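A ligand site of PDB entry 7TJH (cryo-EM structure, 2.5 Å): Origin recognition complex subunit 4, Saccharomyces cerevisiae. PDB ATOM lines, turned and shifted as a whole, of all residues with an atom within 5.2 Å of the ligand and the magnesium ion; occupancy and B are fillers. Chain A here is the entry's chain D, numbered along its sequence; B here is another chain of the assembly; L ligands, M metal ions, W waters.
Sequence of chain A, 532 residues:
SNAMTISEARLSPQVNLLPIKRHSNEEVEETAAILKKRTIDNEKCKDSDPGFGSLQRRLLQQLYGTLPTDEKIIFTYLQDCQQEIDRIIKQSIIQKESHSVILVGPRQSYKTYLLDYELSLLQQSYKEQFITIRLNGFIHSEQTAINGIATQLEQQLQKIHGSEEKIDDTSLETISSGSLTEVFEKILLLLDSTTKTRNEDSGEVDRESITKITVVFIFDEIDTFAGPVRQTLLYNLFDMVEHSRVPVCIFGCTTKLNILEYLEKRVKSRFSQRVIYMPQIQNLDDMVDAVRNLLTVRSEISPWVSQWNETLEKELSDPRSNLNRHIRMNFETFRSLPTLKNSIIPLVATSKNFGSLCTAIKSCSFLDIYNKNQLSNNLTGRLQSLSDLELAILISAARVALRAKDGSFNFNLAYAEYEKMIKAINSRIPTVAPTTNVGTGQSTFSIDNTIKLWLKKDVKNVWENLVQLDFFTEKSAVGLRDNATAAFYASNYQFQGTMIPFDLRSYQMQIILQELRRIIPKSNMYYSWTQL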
ATOM      1  N   TYR A  64     -40.002   3.694   1.614  1.00  0.00           N
ATOM      2  CA  TYR A  64     -38.669   3.231   1.235  1.00  0.00           C
ATOM      3  C   TYR A  64     -37.956   4.167   0.269  1.00  0.00           C
ATOM      4  O   TYR A  64     -36.798   3.930  -0.053  1.00  0.00           O
ATOM      5  CB  TYR A  64     -38.744   1.832   0.618  1.00  0.00           C
ATOM      6  CG  TYR A  64     -38.901   0.734   1.639  1.00  0.00           C
ATOM      7  CD1 TYR A  64     -37.810   0.303   2.392  1.00  0.00           C
ATOM      8  CD2 TYR A  64     -40.126   0.127   1.850  1.00  0.00           C
ATOM      9  CE1 TYR A  64     -37.957  -0.718   3.332  1.00  0.00           C
ATOM     10  CE2 TYR A  64     -40.277  -0.873   2.787  1.00  0.00           C
ATOM     11  CZ  TYR A  64     -39.184  -1.287   3.524  1.00  0.00           C
ATOM     12  OH  TYR A  64     -39.350  -2.287   4.451  1.00  0.00           O
ATOM     13  N   GLY A  65     -38.624   5.235  -0.186  1.00  0.00           N
ATOM     14  CA  GLY A  65     -37.997   6.200  -1.059  1.00  0.00           C
ATOM     15  C   GLY A  65     -37.716   5.714  -2.460  1.00  0.00           C
ATOM     16  O   GLY A  65     -36.868   6.287  -3.142  1.00  0.00           O
ATOM     17  N   THR A  66     -38.413   4.685  -2.915  1.00  0.00           N
ATOM     18  CA  THR A  66     -38.179   4.082  -4.231  1.00  0.00           C
ATOM     19  C   THR A  66     -39.156   4.606  -5.266  1.00  0.00           C
ATOM     20  O   THR A  66     -39.568   3.884  -6.175  1.00  0.00           O
ATOM     21  CB  THR A  66     -38.236   2.564  -4.137  1.00  0.00           C
ATOM     22  OG1 THR A  66     -39.390   2.168  -3.389  1.00  0.00           O
ATOM     23  CG2 THR A  66     -36.977   2.032  -3.464  1.00  0.00           C
ATOM     24  N   LYS A  72     -39.798  12.265  -6.303  1.00  0.00           N
ATOM     25  CA  LYS A  72     -39.031  12.011  -5.093  1.00  0.00           C
ATOM     26  C   LYS A  72     -39.252  13.105  -4.047  1.00  0.00           C
ATOM     27  O   LYS A  72     -39.351  14.288  -4.364  1.00  0.00           O
ATOM     28  CB  LYS A  72     -37.540  11.915  -5.423  1.00  0.00           C
ATOM     29  CG  LYS A  72     -37.090  10.510  -5.787  1.00  0.00           C
ATOM     30  CD  LYS A  72     -36.387   9.841  -4.623  1.00  0.00           C
ATOM     31  CE  LYS A  72     -35.335   8.867  -5.084  1.00  0.00           C
ATOM     32  NZ  LYS A  72     -34.221   8.774  -4.115  1.00  0.00           N
ATOM     33  N   GLY A 105     -22.019  14.883   8.235  1.00  0.00           N
ATOM     34  CA  GLY A 105     -23.255  14.673   8.929  1.00  0.00           C
ATOM     35  C   GLY A 105     -23.291  13.292   9.541  1.00  0.00           C
ATOM     36  O   GLY A 105     -22.494  12.415   9.187  1.00  0.00           O
ATOM     37  N   PRO A 106     -24.225  13.057  10.469  1.00  0.00           N
ATOM     38  CA  PRO A 106     -24.331  11.733  11.093  1.00  0.00           C
ATOM     39  C   PRO A 106     -24.844  10.678  10.130  1.00  0.00           C
ATOM     40  O   PRO A 106     -25.229  10.966   8.989  1.00  0.00           O
ATOM     41  CB  PRO A 106     -25.324  11.957  12.237  1.00  0.00           C
ATOM     42  CG  PRO A 106     -26.001  13.237  11.953  1.00  0.00           C
ATOM     43  CD  PRO A 106     -25.091  14.060  11.109  1.00  0.00           C
ATOM     44  N   ARG A 107     -24.799   9.428  10.584  1.00  0.00           N
ATOM     45  CA  ARG A 107     -25.383   8.328   9.838  1.00  0.00           C
ATOM     46  C   ARG A 107     -26.878   8.543   9.682  1.00  0.00           C
ATOM     47  O   ARG A 107     -27.537   9.077  10.583  1.00  0.00           O
ATOM     48  CB  ARG A 107     -25.102   7.003  10.533  1.00  0.00           C
ATOM     49  CG  ARG A 107     -23.638   6.682  10.706  1.00  0.00           C
ATOM     50  CD  ARG A 107     -23.362   5.212  10.537  1.00  0.00           C
ATOM     51  NE  ARG A 107     -21.931   4.925  10.557  1.00  0.00           N
ATOM     52  CZ  ARG A 107     -21.133   5.027   9.511  1.00  0.00           C
ATOM     53  NH1 ARG A 107     -21.591   5.359   8.312  1.00  0.00           N
ATOM     54  NH2 ARG A 107     -19.833   4.801   9.661  1.00  0.00           N
ATOM     55  N   GLN A 108     -27.399   8.147   8.513  1.00  0.00           N
ATOM     56  CA  GLN A 108     -28.817   8.272   8.133  1.00  0.00           C
ATOM     57  C   GLN A 108     -29.292   9.729   8.152  1.00  0.00           C
ATOM     58  O   GLN A 108     -30.426  10.023   8.501  1.00  0.00           O
ATOM     59  CB  GLN A 108     -29.715   7.387   9.011  1.00  0.00           C
ATOM     60  CG  GLN A 108     -29.300   5.942   9.063  1.00  0.00           C
ATOM     61  CD  GLN A 108     -29.685   5.200   7.803  1.00  0.00           C
ATOM     62  OE1 GLN A 108     -30.860   4.941   7.560  1.00  0.00           O
ATOM     63  NE2 GLN A 108     -28.696   4.858   6.986  1.00  0.00           N
ATOM     64  N   SER A 109     -28.399  10.644   7.770  1.00  0.00           N
ATOM     65  CA  SER A 109     -28.743  12.054   7.662  1.00  0.00           C
ATOM     66  C   SER A 109     -28.758  12.528   6.212  1.00  0.00           C
ATOM     67  O   SER A 109     -28.482  13.692   5.931  1.00  0.00           O
ATOM     68  CB  SER A 109     -27.795  12.917   8.496  1.00  0.00           C
ATOM     69  OG  SER A 109     -26.464  12.855   8.020  1.00  0.00           O
ATOM     70  N   TYR A 110     -29.029  11.601   5.277  1.00  0.00           N
ATOM     71  CA  TYR A 110     -29.392  11.875   3.888  1.00  0.00           C
ATOM     72  C   TYR A 110     -28.228  12.448   3.069  1.00  0.00           C
ATOM     73  O   TYR A 110     -28.426  13.295   2.207  1.00  0.00           O
ATOM     74  CB  TYR A 110     -30.629  12.783   3.773  1.00  0.00           C
ATOM     75  CG  TYR A 110     -31.871  12.203   4.393  1.00  0.00           C
ATOM     76  CD1 TYR A 110     -32.168  12.431   5.735  1.00  0.00           C
ATOM     77  CD2 TYR A 110     -32.750  11.426   3.655  1.00  0.00           C
ATOM     78  CE1 TYR A 110     -33.304  11.903   6.310  1.00  0.00           C
ATOM     79  CE2 TYR A 110     -33.889  10.891   4.222  1.00  0.00           C
ATOM     80  CZ  TYR A 110     -34.161  11.131   5.548  1.00  0.00           C
ATOM     81  OH  TYR A 110     -35.289  10.604   6.119  1.00  0.00           O
ATOM     82  N   LYS A 111     -27.005  11.972   3.317  1.00  0.00           N
ATOM     83  CA  LYS A 111     -25.900  12.339   2.432  1.00  0.00           C
ATOM     84  C   LYS A 111     -25.972  11.555   1.124  1.00  0.00           C
ATOM     85  O   LYS A 111     -25.995  12.137   0.025  1.00  0.00           O
ATOM     86  CB  LYS A 111     -24.568  12.125   3.138  1.00  0.00           C
ATOM     87  CG  LYS A 111     -24.431  12.895   4.442  1.00  0.00           C
ATOM     88  CD  LYS A 111     -22.996  12.926   4.953  1.00  0.00           C
ATOM     89  CE  LYS A 111     -22.524  11.563   5.429  1.00  0.00           C
ATOM     90  NZ  LYS A 111     -23.286  11.079   6.614  1.00  0.00           N
ATOM     91  N   THR A 112     -26.022  10.216   1.224  1.00  0.00           N
ATOM     92  CA  THR A 112     -26.138   9.351   0.048  1.00  0.00           C
ATOM     93  C   THR A 112     -27.464   9.575  -0.667  1.00  0.00           C
ATOM     94  O   THR A 112     -27.520   9.520  -1.901  1.00  0.00           O
ATOM     95  CB  THR A 112     -25.960   7.891   0.458  1.00  0.00           C
ATOM     96  OG1 THR A 112     -24.685   7.731   1.093  1.00  0.00           O
ATOM     97  CG2 THR A 112     -26.040   6.936  -0.719  1.00  0.00           C
ATOM     98  N   TYR A 113     -28.543   9.845   0.087  1.00  0.00           N
ATOM     99  CA  TYR A 113     -29.854  10.074  -0.503  1.00  0.00           C
ATOM    100  C   TYR A 113     -29.851  11.318  -1.392  1.00  0.00           C
ATOM    101  O   TYR A 113     -30.307  11.270  -2.538  1.00  0.00           O
ATOM    102  CB  TYR A 113     -30.907  10.212   0.596  1.00  0.00           C
ATOM    103  CG  TYR A 113     -32.310  10.426   0.095  1.00  0.00           C
ATOM    104  CD1 TYR A 113     -33.073   9.371  -0.373  1.00  0.00           C
ATOM    105  CD2 TYR A 113     -32.882  11.697   0.098  1.00  0.00           C
ATOM    106  CE1 TYR A 113     -34.358   9.562  -0.832  1.00  0.00           C
ATOM    107  CE2 TYR A 113     -34.160  11.904  -0.363  1.00  0.00           C
ATOM    108  CZ  TYR A 113     -34.898  10.836  -0.828  1.00  0.00           C
ATOM    109  OH  TYR A 113     -36.175  11.043  -1.288  1.00  0.00           O
ATOM    110  N   ASP A 116     -27.469  10.739  -4.463  1.00  0.00           N
ATOM    111  CA  ASP A 116     -28.090   9.862  -5.440  1.00  0.00           C
ATOM    112  C   ASP A 116     -29.236  10.557  -6.174  1.00  0.00           C
ATOM    113  O   ASP A 116     -29.425  10.341  -7.369  1.00  0.00           O
ATOM    114  CB  ASP A 116     -28.600   8.596  -4.744  1.00  0.00           C
ATOM    115  CG  ASP A 116     -27.493   7.612  -4.438  1.00  0.00           C
ATOM    116  OD1 ASP A 116     -26.307   7.999  -4.586  1.00  0.00           O
ATOM    117  OD2 ASP A 116     -27.792   6.473  -4.038  1.00  0.00           O
ATOM    118  N   ASP A 220     -17.440   7.777  -0.011  1.00  0.00           N
ATOM    119  CA  ASP A 220     -18.030   7.564   1.300  1.00  0.00           C
ATOM    120  C   ASP A 220     -16.988   7.040   2.278  1.00  0.00           C
ATOM    121  O   ASP A 220     -16.063   6.315   1.895  1.00  0.00           O
ATOM    122  CB  ASP A 220     -19.197   6.581   1.212  1.00  0.00           C
ATOM    123  CG  ASP A 220     -20.222   6.993   0.177  1.00  0.00           C
ATOM    124  OD1 ASP A 220     -20.263   8.191  -0.154  1.00  0.00           O
ATOM    125  OD2 ASP A 220     -20.973   6.120  -0.301  1.00  0.00           O
ATOM    126  N   GLU A 221     -17.155   7.426   3.545  1.00  0.00           N
ATOM    127  CA  GLU A 221     -16.213   7.155   4.643  1.00  0.00           C
ATOM    128  C   GLU A 221     -14.801   7.634   4.304  1.00  0.00           C
ATOM    129  O   GLU A 221     -13.825   6.893   4.374  1.00  0.00           O
ATOM    130  CB  GLU A 221     -16.204   5.668   5.027  1.00  0.00           C
ATOM    131  CG  GLU A 221     -17.582   5.064   5.209  1.00  0.00           C
ATOM    132  CD  GLU A 221     -18.228   5.492   6.515  1.00  0.00           C
ATOM    133  OE1 GLU A 221     -17.486   5.728   7.494  1.00  0.00           O
ATOM    134  OE2 GLU A 221     -19.469   5.573   6.565  1.00  0.00           O
ATOM    135  N   THR A 255     -18.802  11.173   8.928  1.00  0.00           N
ATOM    136  CA  THR A 255     -19.482  11.558  10.160  1.00  0.00           C
ATOM    137  C   THR A 255     -18.594  12.391  11.077  1.00  0.00           C
ATOM    138  O   THR A 255     -19.083  12.889  12.095  1.00  0.00           O
ATOM    139  CB  THR A 255     -19.967  10.314  10.924  1.00  0.00           C
ATOM    140  OG1 THR A 255     -18.847   9.538  11.346  1.00  0.00           O
ATOM    141  CG2 THR A 255     -20.868   9.467  10.050  1.00  0.00           C
ATOM    142  N   PRO A 338     -35.517   7.956   9.853  1.00  0.00           N
ATOM    143  CA  PRO A 338     -35.444   6.504   9.561  1.00  0.00           C
ATOM    144  C   PRO A 338     -35.900   5.611  10.702  1.00  0.00           C
ATOM    145  O   PRO A 338     -36.484   4.545  10.435  1.00  0.00           O
ATOM    146  CB  PRO A 338     -33.966   6.285   9.232  1.00  0.00           C
ATOM    147  CG  PRO A 338     -33.531   7.539   8.673  1.00  0.00           C
ATOM    148  CD  PRO A 338     -34.255   8.604   9.423  1.00  0.00           C
ATOM    149  N   LYS A 341     -39.581   5.657  10.445  1.00  0.00           N
ATOM    150  CA  LYS A 341     -40.002   4.939   9.240  1.00  0.00           C
ATOM    151  C   LYS A 341     -39.962   3.429   9.447  1.00  0.00           C
ATOM    152  O   LYS A 341     -40.837   2.703   8.958  1.00  0.00           O
ATOM    153  CB  LYS A 341     -39.117   5.321   8.055  1.00  0.00           C
ATOM    154  CG  LYS A 341     -39.453   6.648   7.413  1.00  0.00           C
ATOM    155  CD  LYS A 341     -38.792   6.780   6.058  1.00  0.00           C
ATOM    156  CE  LYS A 341     -37.286   6.619   6.153  1.00  0.00           C
ATOM    157  NZ  LYS A 341     -36.647   6.647   4.811  1.00  0.00           N
ATOM    158  N   LYS B 151     -22.930  -1.823   3.778  1.00  0.00           N
ATOM    159  CA  LYS B 151     -22.708  -0.868   2.700  1.00  0.00           C
ATOM    160  C   LYS B 151     -22.467  -1.531   1.352  1.00  0.00           C
ATOM    161  O   LYS B 151     -22.214  -0.823   0.368  1.00  0.00           O
ATOM    162  CB  LYS B 151     -21.561   0.075   3.054  1.00  0.00           C
ATOM    163  CG  LYS B 151     -21.892   1.074   4.142  1.00  0.00           C
ATOM    164  CD  LYS B 151     -23.221   1.765   3.875  1.00  0.00           C
ATOM    165  CE  LYS B 151     -23.457   2.928   4.826  1.00  0.00           C
ATOM    166  NZ  LYS B 151     -24.850   3.441   4.712  1.00  0.00           N
ATOM    167  N   GLU B 154     -24.684  -0.481  -1.877  1.00  0.00           N
ATOM    168  CA  GLU B 154     -24.474   0.797  -2.556  1.00  0.00           C
ATOM    169  C   GLU B 154     -23.476   0.695  -3.698  1.00  0.00           C
ATOM    170  O   GLU B 154     -23.465   1.579  -4.565  1.00  0.00           O
ATOM    171  CB  GLU B 154     -24.016   1.864  -1.562  1.00  0.00           C
ATOM    172  CG  GLU B 154     -25.162   2.673  -0.964  1.00  0.00           C
ATOM    173  CD  GLU B 154     -24.941   3.019   0.500  1.00  0.00           C
ATOM    174  OE1 GLU B 154     -23.839   3.495   0.833  1.00  0.00           O
ATOM    175  OE2 GLU B 154     -25.877   2.837   1.304  1.00  0.00           O
ATOM    176  N   LYS B 158     -27.693  -0.195  -9.657  1.00  0.00           N
ATOM    177  CA  LYS B 158     -29.021   0.147  -9.177  1.00  0.00           C
ATOM    178  C   LYS B 158     -30.142  -0.306 -10.098  1.00  0.00           C
ATOM    179  O   LYS B 158     -31.234  -0.614  -9.627  1.00  0.00           O
ATOM    180  CB  LYS B 158     -29.119   1.666  -8.976  1.00  0.00           C
ATOM    181  CG  LYS B 158     -28.776   2.126  -7.573  1.00  0.00           C
ATOM    182  CD  LYS B 158     -28.568   3.633  -7.537  1.00  0.00           C
ATOM    183  CE  LYS B 158     -28.859   4.187  -6.164  1.00  0.00           C
ATOM    184  NZ  LYS B 158     -29.831   5.322  -6.235  1.00  0.00           N
ATOM    185  N   HIS B 182     -27.142   2.933  12.211  1.00  0.00           N
ATOM    186  CA  HIS B 182     -27.419   2.577  10.823  1.00  0.00           C
ATOM    187  C   HIS B 182     -28.913   2.451  10.540  1.00  0.00           C
ATOM    188  O   HIS B 182     -29.300   2.470   9.373  1.00  0.00           O
ATOM    189  CB  HIS B 182     -26.704   1.291  10.461  1.00  0.00           C
ATOM    190  CG  HIS B 182     -25.238   1.460  10.168  1.00  0.00           C
ATOM    191  ND1 HIS B 182     -24.778   2.014   8.991  1.00  0.00           N
ATOM    192  CD2 HIS B 182     -24.144   1.196  10.913  1.00  0.00           C
ATOM    193  CE1 HIS B 182     -23.458   2.052   9.021  1.00  0.00           C
ATOM    194  NE2 HIS B 182     -23.046   1.563  10.177  1.00  0.00           N
HETATM  195  P1  LIG L   1     -24.044   7.091   6.346  1.00  0.00           P
HETATM  196  O1  LIG L   1     -24.263   5.925   7.240  1.00  0.00           O
HETATM  197  O2  LIG L   1     -23.180   8.180   6.946  1.00  0.00           O
HETATM  198  O3  LIG L   1     -23.477   6.698   4.991  1.00  0.00           O
HETATM  199  P2  LIG L   1     -26.043   8.761   4.925  1.00  0.00           P
HETATM  200  O4  LIG L   1     -25.425   8.582   3.617  1.00  0.00           O
HETATM  201  O5  LIG L   1     -25.992  10.179   5.492  1.00  0.00           O
HETATM  202  O6  LIG L   1     -25.417   7.816   6.008  1.00  0.00           O
HETATM  203  P3  LIG L   1     -28.638   7.773   3.940  1.00  0.00           P
HETATM  204  O7  LIG L   1     -28.941   8.773   2.899  1.00  0.00           O
HETATM  205  O8  LIG L   1     -28.105   6.462   3.382  1.00  0.00           O
HETATM  206  O9  LIG L   1     -27.568   8.315   4.961  1.00  0.00           O
HETATM  207  O10 LIG L   1     -29.858   7.465   4.886  1.00  0.00           O
HETATM  208  C1  LIG L   1     -31.011   8.336   4.940  1.00  0.00           C
HETATM  209  C2  LIG L   1     -32.230   7.611   4.408  1.00  0.00           C
HETATM  210  O11 LIG L   1     -32.233   7.663   2.963  1.00  0.00           O
HETATM  211  C3  LIG L   1     -32.350   6.139   4.800  1.00  0.00           C
HETATM  212  O12 LIG L   1     -33.670   5.827   5.241  1.00  0.00           O
HETATM  213  C4  LIG L   1     -31.975   5.395   3.512  1.00  0.00           C
HETATM  214  O13 LIG L   1     -32.661   4.148   3.384  1.00  0.00           O
HETATM  215  C5  LIG L   1     -32.438   6.368   2.441  1.00  0.00           C
HETATM  216  N1  LIG L   1     -31.702   6.265   1.184  1.00  0.00           N
HETATM  217  C6  LIG L   1     -30.351   6.369   1.016  1.00  0.00           C
HETATM  218  N2  LIG L   1     -29.953   6.231  -0.228  1.00  0.00           N
HETATM  219  C7  LIG L   1     -31.139   6.020  -0.921  1.00  0.00           C
HETATM  220  C8  LIG L   1     -31.417   5.797  -2.288  1.00  0.00           C
HETATM  221  N3  LIG L   1     -30.482   5.756  -3.237  1.00  0.00           N
HETATM  222  N4  LIG L   1     -32.707   5.623  -2.652  1.00  0.00           N
HETATM  223  C9  LIG L   1     -33.651   5.664  -1.700  1.00  0.00           C
HETATM  224  N5  LIG L   1     -33.512   5.859  -0.393  1.00  0.00           N
HETATM  225  C10 LIG L   1     -32.226   6.031  -0.067  1.00  0.00           C
HETATM  226 MG    MG M   1     -24.199   6.959   2.988  1.00  0.00          MG
HETATM  227  O   HOH W   1     -35.680   6.674   1.553  1.00  0.00           O
HETATM  228  O   HOH W   2     -28.816   4.051   3.761  1.00  0.00           O
HETATM  229  O   HOH W   3     -20.918   4.998   4.353  1.00  0.00           O
HETATM  230  O   HOH W   4     -25.893   5.672   3.070  1.00  0.00           O
HETATM  231  O   HOH W   5     -20.413   7.761   4.332  1.00  0.00           O
HETATM  232  O   HOH W   6     -20.440   8.741   6.730  1.00  0.00           O
HETATM  233  O   HOH W   7     -22.958   8.688   2.975  1.00  0.00           O
HETATM  234  O   HOH W   8     -22.822   5.676   1.940  1.00  0.00           O
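The backbone NH (N) of Thr 112 sits close to an oxygen (O4) of the ligand, 3.0 Å away.
The side-chain carboxylate of Asp 116 sits at hydrogen-bond distance from a nitrogen (N3) of the ligand (2.9 Å).
An oxygen (O5) of the ligand sits at hydrogen-bond distance from the backbone NH of Lys 111 (3.0 Å).
NZ of Lys 111 lies within salt-bridge range of O2 of the ligand (2.9 Å).
An oxygen (O1) of the ligand lies within salt-bridge range of the guanidinium group (NH1) of Arg 107, 2.9 Å away.
The backbone NH (N) of Tyr 113 sits at hydrogen-bond distance from an oxygen (O7) of the ligand, 3.0 Å away.
NZ of Lys 341 is in hydrogen-bond range of O12 of the ligand, at 3.1 Å.
An oxygen (O6) of the ligand sits at hydrogen-bond distance from the backbone NH (N) of Gln 108.
N of Tyr 110 is in hydrogen-bond range of O5 of the ligand, 3.4 Å away.
The backbone NH (N) of Ser 109 is in hydrogen-bond range of an oxygen (O5) of the ligand, 3.3 Å away.
The side-chain amino group (NZ) of Lys 151 of chain B lies within salt-bridge range of an oxygen (O1) of the ligand, 3.6 Å away.
The side-chain carboxylate (OD2) of Asp 116 lies within salt-bridge range of the side-chain amino group (NZ) of Lys 158 of chain B (3.2 Å).
The backbone carbonyl oxygen of Pro 106 sits at hydrogen-bond distance from the side-chain amino group of Lys 111, at 3.1 Å.
The backbone carbonyl oxygen (O) of Gly 105 is in hydrogen-bond range of the side-chain amino group (NZ) of Lys 111 (3.0 Å).
NH1 of Arg 107 is in salt-bridge range of OE2 of Glu 221 (2.8 Å).
O of His 182 of chain B sits close to NE2 of Gln 108 (3.4 Å).
The backbone carbonyl oxygen of Pro 106 lies within hydrogen-bond range of the side-chain hydroxyl of Ser 109 (2.5 Å).
The side-chain carboxylate (OE2) of Glu 154 of chain B lies within salt-bridge range of the side-chain amino group (NZ) of Lys 151 of chain B, at 3.6 Å.
NZ of Lys 158 of chain B sits close to N3 of the ligand.
Merely in contact with the ligand: Gly 65 (3.6 Å), Pro 106 (3.7 Å), Lys 72 (3.8 Å), Tyr 64 (3.8 Å) and Pro 338 (3.8 Å).
Hydrophobic or aromatic side chains that line the ligand: Tyr 110, Tyr 113 and Pro 338.
Within 4 Å of the ligand: Tyr 64, Gly 65, Lys 72, Pro 106, Arg 107, Gln 108, Ser 109, Tyr 110, Lys 111, Thr 112, Tyr 113, Asp 116, Pro 338, Lys 341, Lys 151 of chain B and Lys 158 of chain B.
The nearest printed residue that does not touch the ligand is Thr 255 (4.1 Å).
Lys 151 of chain B touches the magnesium ion (NZ to MG, 3.97 Å).
The nearest printed residue that does not touch the magnesium ion is Glu 154 of chain B (4.1 Å).
The magnesium ion is bound by OG1 of Thr 112 (2.1 Å).
The magnesium ion is bound by water W7.
O4 of the ligand is bound to the magnesium ion (2.1 Å).
The magnesium ion is bound by water W4 (2.1 Å).
An oxygen (O3) of the ligand binds the magnesium ion (2.1 Å).
Water W8 is bound to the magnesium ion (2.2 Å).
The magnesium ion has six donor atoms within binding distance.
Water W4 bridges the side-chain amino group (NZ) of Lys 151 of chain B (3.0 Å) and the side-chain carboxylate (OE2) of Glu 154 of chain B (3.3 Å).
Water W8 lies within hydrogen-bond range of the side-chain carboxylate of Glu 154 of chain B (2.6 Å) and the side-chain carboxylate of Asp 220 (2.9 Å).
Water W2 lies within hydrogen-bond range of an oxygen (O8) of the ligand (2.5 Å) and the side-chain amide nitrogen (NE2) of Gln 108 (3.3 Å).
Water W6 bridges O2 of the ligand (2.8 Å) and OE2 of Glu 221 (3.3 Å).
Water W1 lies within hydrogen-bond range of a nitrogen (N5) of the ligand (3.0 Å), the backbone carbonyl oxygen (O) of Tyr 64 (3.4 Å) and the side-chain amino group (NZ) of Lys 341 (3.4 Å).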
